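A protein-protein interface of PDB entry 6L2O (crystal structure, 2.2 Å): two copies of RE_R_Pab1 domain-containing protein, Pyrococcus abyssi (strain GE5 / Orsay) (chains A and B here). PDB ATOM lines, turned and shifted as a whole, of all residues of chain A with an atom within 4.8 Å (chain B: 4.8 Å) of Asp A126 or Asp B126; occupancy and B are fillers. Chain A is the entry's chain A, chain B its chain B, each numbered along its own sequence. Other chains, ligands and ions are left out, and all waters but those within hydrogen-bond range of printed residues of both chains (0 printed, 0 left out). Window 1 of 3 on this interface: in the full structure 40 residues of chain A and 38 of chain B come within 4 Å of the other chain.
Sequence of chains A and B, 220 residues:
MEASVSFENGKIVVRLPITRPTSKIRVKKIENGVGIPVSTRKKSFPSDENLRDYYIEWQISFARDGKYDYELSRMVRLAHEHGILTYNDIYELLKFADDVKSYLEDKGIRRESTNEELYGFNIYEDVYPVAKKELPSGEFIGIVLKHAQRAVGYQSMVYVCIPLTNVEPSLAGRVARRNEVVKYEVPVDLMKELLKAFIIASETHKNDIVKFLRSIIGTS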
ATOM      1  N   ARG A 110      21.315 -23.366  -9.575  1.00  0.00           N
ATOM      2  CA  ARG A 110      22.158 -23.522  -8.402  1.00  0.00           C
ATOM      3  C   ARG A 110      21.839 -24.838  -7.707  1.00  0.00           C
ATOM      4  O   ARG A 110      20.703 -25.316  -7.733  1.00  0.00           O
ATOM      5  CB  ARG A 110      22.002 -22.334  -7.417  1.00  0.00           C
ATOM      6  CG  ARG A 110      20.736 -22.335  -6.545  1.00  0.00           C
ATOM      7  CD  ARG A 110      20.450 -20.949  -5.929  1.00  0.00           C
ATOM      8  NE  ARG A 110      19.186 -20.929  -5.188  1.00  0.00           N
ATOM      9  CZ  ARG A 110      18.112 -20.254  -5.592  1.00  0.00           C
ATOM     10  NH1 ARG A 110      18.164 -19.573  -6.730  1.00  0.00           N
ATOM     11  NH2 ARG A 110      16.987 -20.272  -4.886  1.00  0.00           N
ATOM     12  N   ARG A 111      22.867 -25.438  -7.118  1.00  0.00           N
ATOM     13  CA  ARG A 111      22.705 -26.607  -6.266  1.00  0.00           C
ATOM     14  C   ARG A 111      22.820 -26.140  -4.823  1.00  0.00           C
ATOM     15  O   ARG A 111      23.879 -25.665  -4.405  1.00  0.00           O
ATOM     16  CB  ARG A 111      23.753 -27.675  -6.577  1.00  0.00           C
ATOM     17  CG  ARG A 111      23.861 -28.734  -5.495  1.00  0.00           C
ATOM     18  CD  ARG A 111      24.568 -29.974  -5.995  1.00  0.00           C
ATOM     19  NE  ARG A 111      23.820 -30.622  -7.059  1.00  0.00           N
ATOM     20  CZ  ARG A 111      24.179 -31.760  -7.639  1.00  0.00           C
ATOM     21  NH1 ARG A 111      25.293 -32.376  -7.265  1.00  0.00           N
ATOM     22  NH2 ARG A 111      23.428 -32.273  -8.600  1.00  0.00           N
ATOM     23  N   TYR A 124      20.797 -32.818  -1.841  1.00  0.00           N
ATOM     24  CA  TYR A 124      20.910 -31.495  -2.435  1.00  0.00           C
ATOM     25  C   TYR A 124      19.608 -31.146  -3.144  1.00  0.00           C
ATOM     26  O   TYR A 124      18.832 -32.026  -3.527  1.00  0.00           O
ATOM     27  CB  TYR A 124      22.067 -31.419  -3.438  1.00  0.00           C
ATOM     28  CG  TYR A 124      23.450 -31.498  -2.832  1.00  0.00           C
ATOM     29  CD1 TYR A 124      23.928 -30.489  -2.007  1.00  0.00           C
ATOM     30  CD2 TYR A 124      24.291 -32.572  -3.110  1.00  0.00           C
ATOM     31  CE1 TYR A 124      25.204 -30.555  -1.461  1.00  0.00           C
ATOM     32  CE2 TYR A 124      25.564 -32.648  -2.568  1.00  0.00           C
ATOM     33  CZ  TYR A 124      26.010 -31.636  -1.749  1.00  0.00           C
ATOM     34  OH  TYR A 124      27.272 -31.700  -1.220  1.00  0.00           O
ATOM     35  N   GLU A 125      19.384 -29.846  -3.333  1.00  0.00           N
ATOM     36  CA  GLU A 125      18.242 -29.347  -4.093  1.00  0.00           C
ATOM     37  C   GLU A 125      18.754 -28.530  -5.270  1.00  0.00           C
ATOM     38  O   GLU A 125      19.348 -27.462  -5.077  1.00  0.00           O
ATOM     39  CB  GLU A 125      17.318 -28.508  -3.217  1.00  0.00           C
ATOM     40  CG  GLU A 125      17.133 -29.055  -1.839  1.00  0.00           C
ATOM     41  CD  GLU A 125      15.776 -28.734  -1.264  1.00  0.00           C
ATOM     42  OE1 GLU A 125      15.050 -29.675  -0.881  1.00  0.00           O
ATOM     43  OE2 GLU A 125      15.435 -27.537  -1.195  1.00  0.00           O
ATOM     44  N   ASP A 126      18.525 -29.031  -6.482  1.00  0.00           N
ATOM     45  CA  ASP A 126      18.848 -28.310  -7.706  1.00  0.00           C
ATOM     46  C   ASP A 126      17.667 -27.416  -8.066  1.00  0.00           C
ATOM     47  O   ASP A 126      16.550 -27.905  -8.270  1.00  0.00           O
ATOM     48  CB  ASP A 126      19.164 -29.280  -8.845  1.00  0.00           C
ATOM     49  CG  ASP A 126      20.490 -30.001  -8.649  1.00  0.00           C
ATOM     50  OD1 ASP A 126      20.714 -31.028  -9.325  1.00  0.00           O
ATOM     51  OD2 ASP A 126      21.309 -29.550  -7.816  1.00  0.00           O
ATOM     52  N   VAL A 127      17.909 -26.111  -8.135  1.00  0.00           N
ATOM     53  CA  VAL A 127      16.856 -25.119  -8.314  1.00  0.00           C
ATOM     54  C   VAL A 127      16.950 -24.566  -9.730  1.00  0.00           C
ATOM     55  O   VAL A 127      17.951 -23.935 -10.098  1.00  0.00           O
ATOM     56  CB  VAL A 127      16.953 -24.002  -7.264  1.00  0.00           C
ATOM     57  CG1 VAL A 127      15.878 -22.954  -7.504  1.00  0.00           C
ATOM     58  CG2 VAL A 127      16.816 -24.589  -5.870  1.00  0.00           C
ATOM     59  N   TYR A 128      15.913 -24.812 -10.528  1.00  0.00           N
ATOM     60  CA  TYR A 128      15.854 -24.351 -11.904  1.00  0.00           C
ATOM     61  C   TYR A 128      14.800 -23.268 -12.030  1.00  0.00           C
ATOM     62  O   TYR A 128      13.674 -23.445 -11.542  1.00  0.00           O
ATOM     63  CB  TYR A 128      15.535 -25.509 -12.858  1.00  0.00           C
ATOM     64  CG  TYR A 128      16.646 -26.535 -12.980  1.00  0.00           C
ATOM     65  CD1 TYR A 128      17.496 -26.545 -14.077  1.00  0.00           C
ATOM     66  CD2 TYR A 128      16.837 -27.497 -11.996  1.00  0.00           C
ATOM     67  CE1 TYR A 128      18.510 -27.484 -14.185  1.00  0.00           C
ATOM     68  CE2 TYR A 128      17.850 -28.439 -12.098  1.00  0.00           C
ATOM     69  CZ  TYR A 128      18.681 -28.426 -13.186  1.00  0.00           C
ATOM     70  OH  TYR A 128      19.676 -29.362 -13.275  1.00  0.00           O
ATOM     71  N   VAL A 130      12.032 -20.937 -13.972  1.00  0.00           N
ATOM     72  CA  VAL A 130      11.134 -20.938 -15.120  1.00  0.00           C
ATOM     73  C   VAL A 130      10.307 -19.660 -15.102  1.00  0.00           C
ATOM     74  O   VAL A 130      10.086 -19.046 -14.055  1.00  0.00           O
ATOM     75  CB  VAL A 130      10.195 -22.169 -15.169  1.00  0.00           C
ATOM     76  CG1 VAL A 130      10.962 -23.461 -14.949  1.00  0.00           C
ATOM     77  CG2 VAL A 130       9.066 -22.026 -14.171  1.00  0.00           C
ATOM     78  N   ARG B 110       9.179 -30.012  -6.917  1.00  0.00           N
ATOM     79  CA  ARG B 110       8.337 -28.902  -6.499  1.00  0.00           C
ATOM     80  C   ARG B 110       8.513 -27.721  -7.443  1.00  0.00           C
ATOM     81  O   ARG B 110       9.628 -27.426  -7.885  1.00  0.00           O
ATOM     82  CB  ARG B 110       8.667 -28.462  -5.069  1.00  0.00           C
ATOM     83  CG  ARG B 110       8.367 -29.499  -3.996  1.00  0.00           C
ATOM     84  CD  ARG B 110       9.628 -29.856  -3.216  1.00  0.00           C
ATOM     85  NE  ARG B 110      10.575 -30.609  -4.036  1.00  0.00           N
ATOM     86  CZ  ARG B 110      11.820 -30.905  -3.670  1.00  0.00           C
ATOM     87  NH1 ARG B 110      12.285 -30.516  -2.489  1.00  0.00           N
ATOM     88  NH2 ARG B 110      12.599 -31.595  -4.489  1.00  0.00           N
ATOM     89  N   ARG B 111       7.408 -27.050  -7.751  1.00  0.00           N
ATOM     90  CA  ARG B 111       7.425 -25.757  -8.428  1.00  0.00           C
ATOM     91  C   ARG B 111       6.958 -24.729  -7.405  1.00  0.00           C
ATOM     92  O   ARG B 111       5.761 -24.615  -7.128  1.00  0.00           O
ATOM     93  CB  ARG B 111       6.542 -25.757  -9.672  1.00  0.00           C
ATOM     94  CG  ARG B 111       6.309 -24.363 -10.253  1.00  0.00           C
ATOM     95  CD  ARG B 111       5.934 -24.420 -11.721  1.00  0.00           C
ATOM     96  NE  ARG B 111       7.043 -24.870 -12.557  1.00  0.00           N
ATOM     97  CZ  ARG B 111       6.931 -25.156 -13.849  1.00  0.00           C
ATOM     98  NH1 ARG B 111       5.756 -25.040 -14.455  1.00  0.00           N
ATOM     99  NH2 ARG B 111       7.991 -25.558 -14.535  1.00  0.00           N
ATOM    100  N   TYR B 124       9.032 -18.644 -11.515  1.00  0.00           N
ATOM    101  CA  TYR B 124       8.907 -19.747 -10.578  1.00  0.00           C
ATOM    102  C   TYR B 124      10.273 -20.392 -10.392  1.00  0.00           C
ATOM    103  O   TYR B 124      11.253 -20.024 -11.046  1.00  0.00           O
ATOM    104  CB  TYR B 124       7.870 -20.776 -11.057  1.00  0.00           C
ATOM    105  CG  TYR B 124       6.473 -20.203 -11.208  1.00  0.00           C
ATOM    106  CD1 TYR B 124       5.500 -20.429 -10.244  1.00  0.00           C
ATOM    107  CD2 TYR B 124       6.133 -19.432 -12.313  1.00  0.00           C
ATOM    108  CE1 TYR B 124       4.223 -19.901 -10.377  1.00  0.00           C
ATOM    109  CE2 TYR B 124       4.862 -18.900 -12.450  1.00  0.00           C
ATOM    110  CZ  TYR B 124       3.911 -19.141 -11.482  1.00  0.00           C
ATOM    111  OH  TYR B 124       2.645 -18.619 -11.616  1.00  0.00           O
ATOM    112  N   GLU B 125      10.334 -21.361  -9.481  1.00  0.00           N
ATOM    113  CA  GLU B 125      11.543 -22.148  -9.274  1.00  0.00           C
ATOM    114  C   GLU B 125      11.149 -23.611  -9.173  1.00  0.00           C
ATOM    115  O   GLU B 125      10.291 -23.968  -8.359  1.00  0.00           O
ATOM    116  CB  GLU B 125      12.293 -21.699  -8.013  1.00  0.00           C
ATOM    117  CG  GLU B 125      13.111 -20.427  -8.195  1.00  0.00           C
ATOM    118  CD  GLU B 125      13.907 -20.066  -6.942  1.00  0.00           C
ATOM    119  OE1 GLU B 125      13.396 -20.307  -5.827  1.00  0.00           O
ATOM    120  OE2 GLU B 125      15.038 -19.545  -7.073  1.00  0.00           O
ATOM    121  N   ASP B 126      11.759 -24.447 -10.011  1.00  0.00           N
ATOM    122  CA  ASP B 126      11.605 -25.892  -9.923  1.00  0.00           C
ATOM    123  C   ASP B 126      12.734 -26.456  -9.070  1.00  0.00           C
ATOM    124  O   ASP B 126      13.905 -26.127  -9.289  1.00  0.00           O
ATOM    125  CB  ASP B 126      11.619 -26.529 -11.314  1.00  0.00           C
ATOM    126  CG  ASP B 126      10.357 -26.229 -12.111  1.00  0.00           C
ATOM    127  OD1 ASP B 126       9.308 -25.944 -11.494  1.00  0.00           O
ATOM    128  OD2 ASP B 126      10.422 -26.271 -13.359  1.00  0.00           O
ATOM    129  N   VAL B 127      12.383 -27.299  -8.106  1.00  0.00           N
ATOM    130  CA  VAL B 127      13.327 -27.834  -7.132  1.00  0.00           C
ATOM    131  C   VAL B 127      13.443 -29.336  -7.361  1.00  0.00           C
ATOM    132  O   VAL B 127      12.515 -30.094  -7.053  1.00  0.00           O
ATOM    133  CB  VAL B 127      12.896 -27.519  -5.693  1.00  0.00           C
ATOM    134  CG1 VAL B 127      13.923 -28.050  -4.696  1.00  0.00           C
ATOM    135  CG2 VAL B 127      12.699 -26.017  -5.516  1.00  0.00           C
ATOM    136  N   TYR B 128      14.586 -29.771  -7.895  1.00  0.00           N
ATOM    137  CA  TYR B 128      14.830 -31.184  -8.152  1.00  0.00           C
ATOM    138  C   TYR B 128      15.748 -31.734  -7.075  1.00  0.00           C
ATOM    139  O   TYR B 128      16.845 -31.189  -6.882  1.00  0.00           O
ATOM    140  CB  TYR B 128      15.463 -31.384  -9.525  1.00  0.00           C
ATOM    141  CG  TYR B 128      14.509 -31.218 -10.682  1.00  0.00           C
ATOM    142  CD1 TYR B 128      14.034 -29.961 -11.042  1.00  0.00           C
ATOM    143  CD2 TYR B 128      14.089 -32.315 -11.422  1.00  0.00           C
ATOM    144  CE1 TYR B 128      13.161 -29.804 -12.099  1.00  0.00           C
ATOM    145  CE2 TYR B 128      13.218 -32.167 -12.484  1.00  0.00           C
ATOM    146  CZ  TYR B 128      12.758 -30.908 -12.816  1.00  0.00           C
ATOM    147  OH  TYR B 128      11.887 -30.748 -13.871  1.00  0.00           O
ATOM    148  N   VAL B 130      18.382 -34.409  -5.268  1.00  0.00           N
ATOM    149  CA  VAL B 130      19.393 -35.384  -5.659  1.00  0.00           C
ATOM    150  C   VAL B 130      20.089 -35.901  -4.410  1.00  0.00           C
ATOM    151  O   VAL B 130      20.379 -35.140  -3.479  1.00  0.00           O
ATOM    152  CB  VAL B 130      20.424 -34.801  -6.656  1.00  0.00           C
ATOM    153  CG1 VAL B 130      19.750 -34.393  -7.968  1.00  0.00           C
ATOM    154  CG2 VAL B 130      21.164 -33.631  -6.052  1.00  0.00           C
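The guanidinium group of Arg A110 is in salt-bridge range of the side-chain carboxylate of Glu B125, 3.0 Å away.
The backbone NH (N) of Tyr A124 sits at hydrogen-bond distance from the backbone carbonyl oxygen (O) of Val B130.
The guanidinium group of Arg B110 lies within salt-bridge range of the side-chain carboxylate of Glu A125, 3.3 Å away.
O of Asp A126 lies within hydrogen-bond range of N of Tyr B128 (2.7 Å).
N of Asp B126 sits at hydrogen-bond distance from O of Tyr A128 (2.6 Å).
O of Val A130 is in hydrogen-bond range of N of Tyr B124, at 2.8 Å.
The backbone carbonyl oxygen of Asp A126 sits close to the backbone carbonyl oxygen of Asp B126 (3.3 Å).
N of Val A127 lies within hydrogen-bond range of O of Arg A110 (2.9 Å).
The guanidinium group (NE) of Arg A111 is in salt-bridge range of the side-chain carboxylate (OD2) of Asp A126 (2.8 Å).
The backbone carbonyl oxygen (O) of Arg B110 is in hydrogen-bond range of the backbone NH (N) of Val B127, 2.8 Å away.
NE of Arg B111 lies within salt-bridge range of OD1 of Asp B126 (2.7 Å).
Arg A111 touches Val B130 (NH2 to CG2, 3.7 Å).
O of Tyr A124 touches O of Tyr B128, at 3.99 Å.
CG1 of Val B127 touches CB of Glu A125, 3.7 Å away.
Asp A126 touches Val B127 (O to CA, 3.4 Å).
Asp A126 touches Val B130 (OD1 to CG1, 3.8 Å).
CG1 of Val A127 touches OE2 of Glu B125, 3.5 Å away.
O of Asp B126 touches CA of Val A127 (3.3 Å).
Glu B125 touches Tyr A128 (CA to O, 3.4 Å).
Tyr B128 touches Tyr A128 (CD1 to CD2, 3.9 Å).
NH2 of Arg B111 touches CG1 of Val A130, at 3.7 Å.
Asp A126 touches four residues of chain B.
Printed residues of chain A within 4 Å of Glu B125: Arg A110 (3.0 Å), Val A127 (3.5 Å) and Tyr A128 (3.4 Å).
Of the printed residues of chain B, Glu A125 touches Arg B110 (3.3 Å), Val B127 (3.7 Å) and Tyr B128 (3.6 Å).
Printed residues of chain B within 4 Å of Val A127: Glu B125 (3.5 Å) and Asp B126 (3.3 Å).
Printed residues of chain A within 4 Å of Tyr B128: Tyr A124, Glu A125, Asp A126 and Tyr A128.
The nearest printed residue of chain B that does not touch Asp A126 is Arg B110 (6.6 Å).
The nearest printed residue of chain A that does not touch Asp B126 is Glu A125 (6.7 Å).
Hydrophobic or aromatic side chains of chain A that line the printed part of chain B: Tyr A124, Val A127, Tyr A128 and Val A130.
Among the printed residues, 19 pairs touch across the chains.
Tyr A124 touches Val B130, and with the chains exchanged Val A130 touches Tyr B124.
Glu A125 touches Tyr B128, and with the chains exchanged Tyr A128 touches Glu B125.
Asp A126 touches its own counterpart, Asp B126.
Tyr A128 touches its own counterpart, Tyr B128.
8 positions are printed for both chains.
Of the 19 pairs that touch across the chains among the printed residues, 18 have their exchanged pair printed and touching as well.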
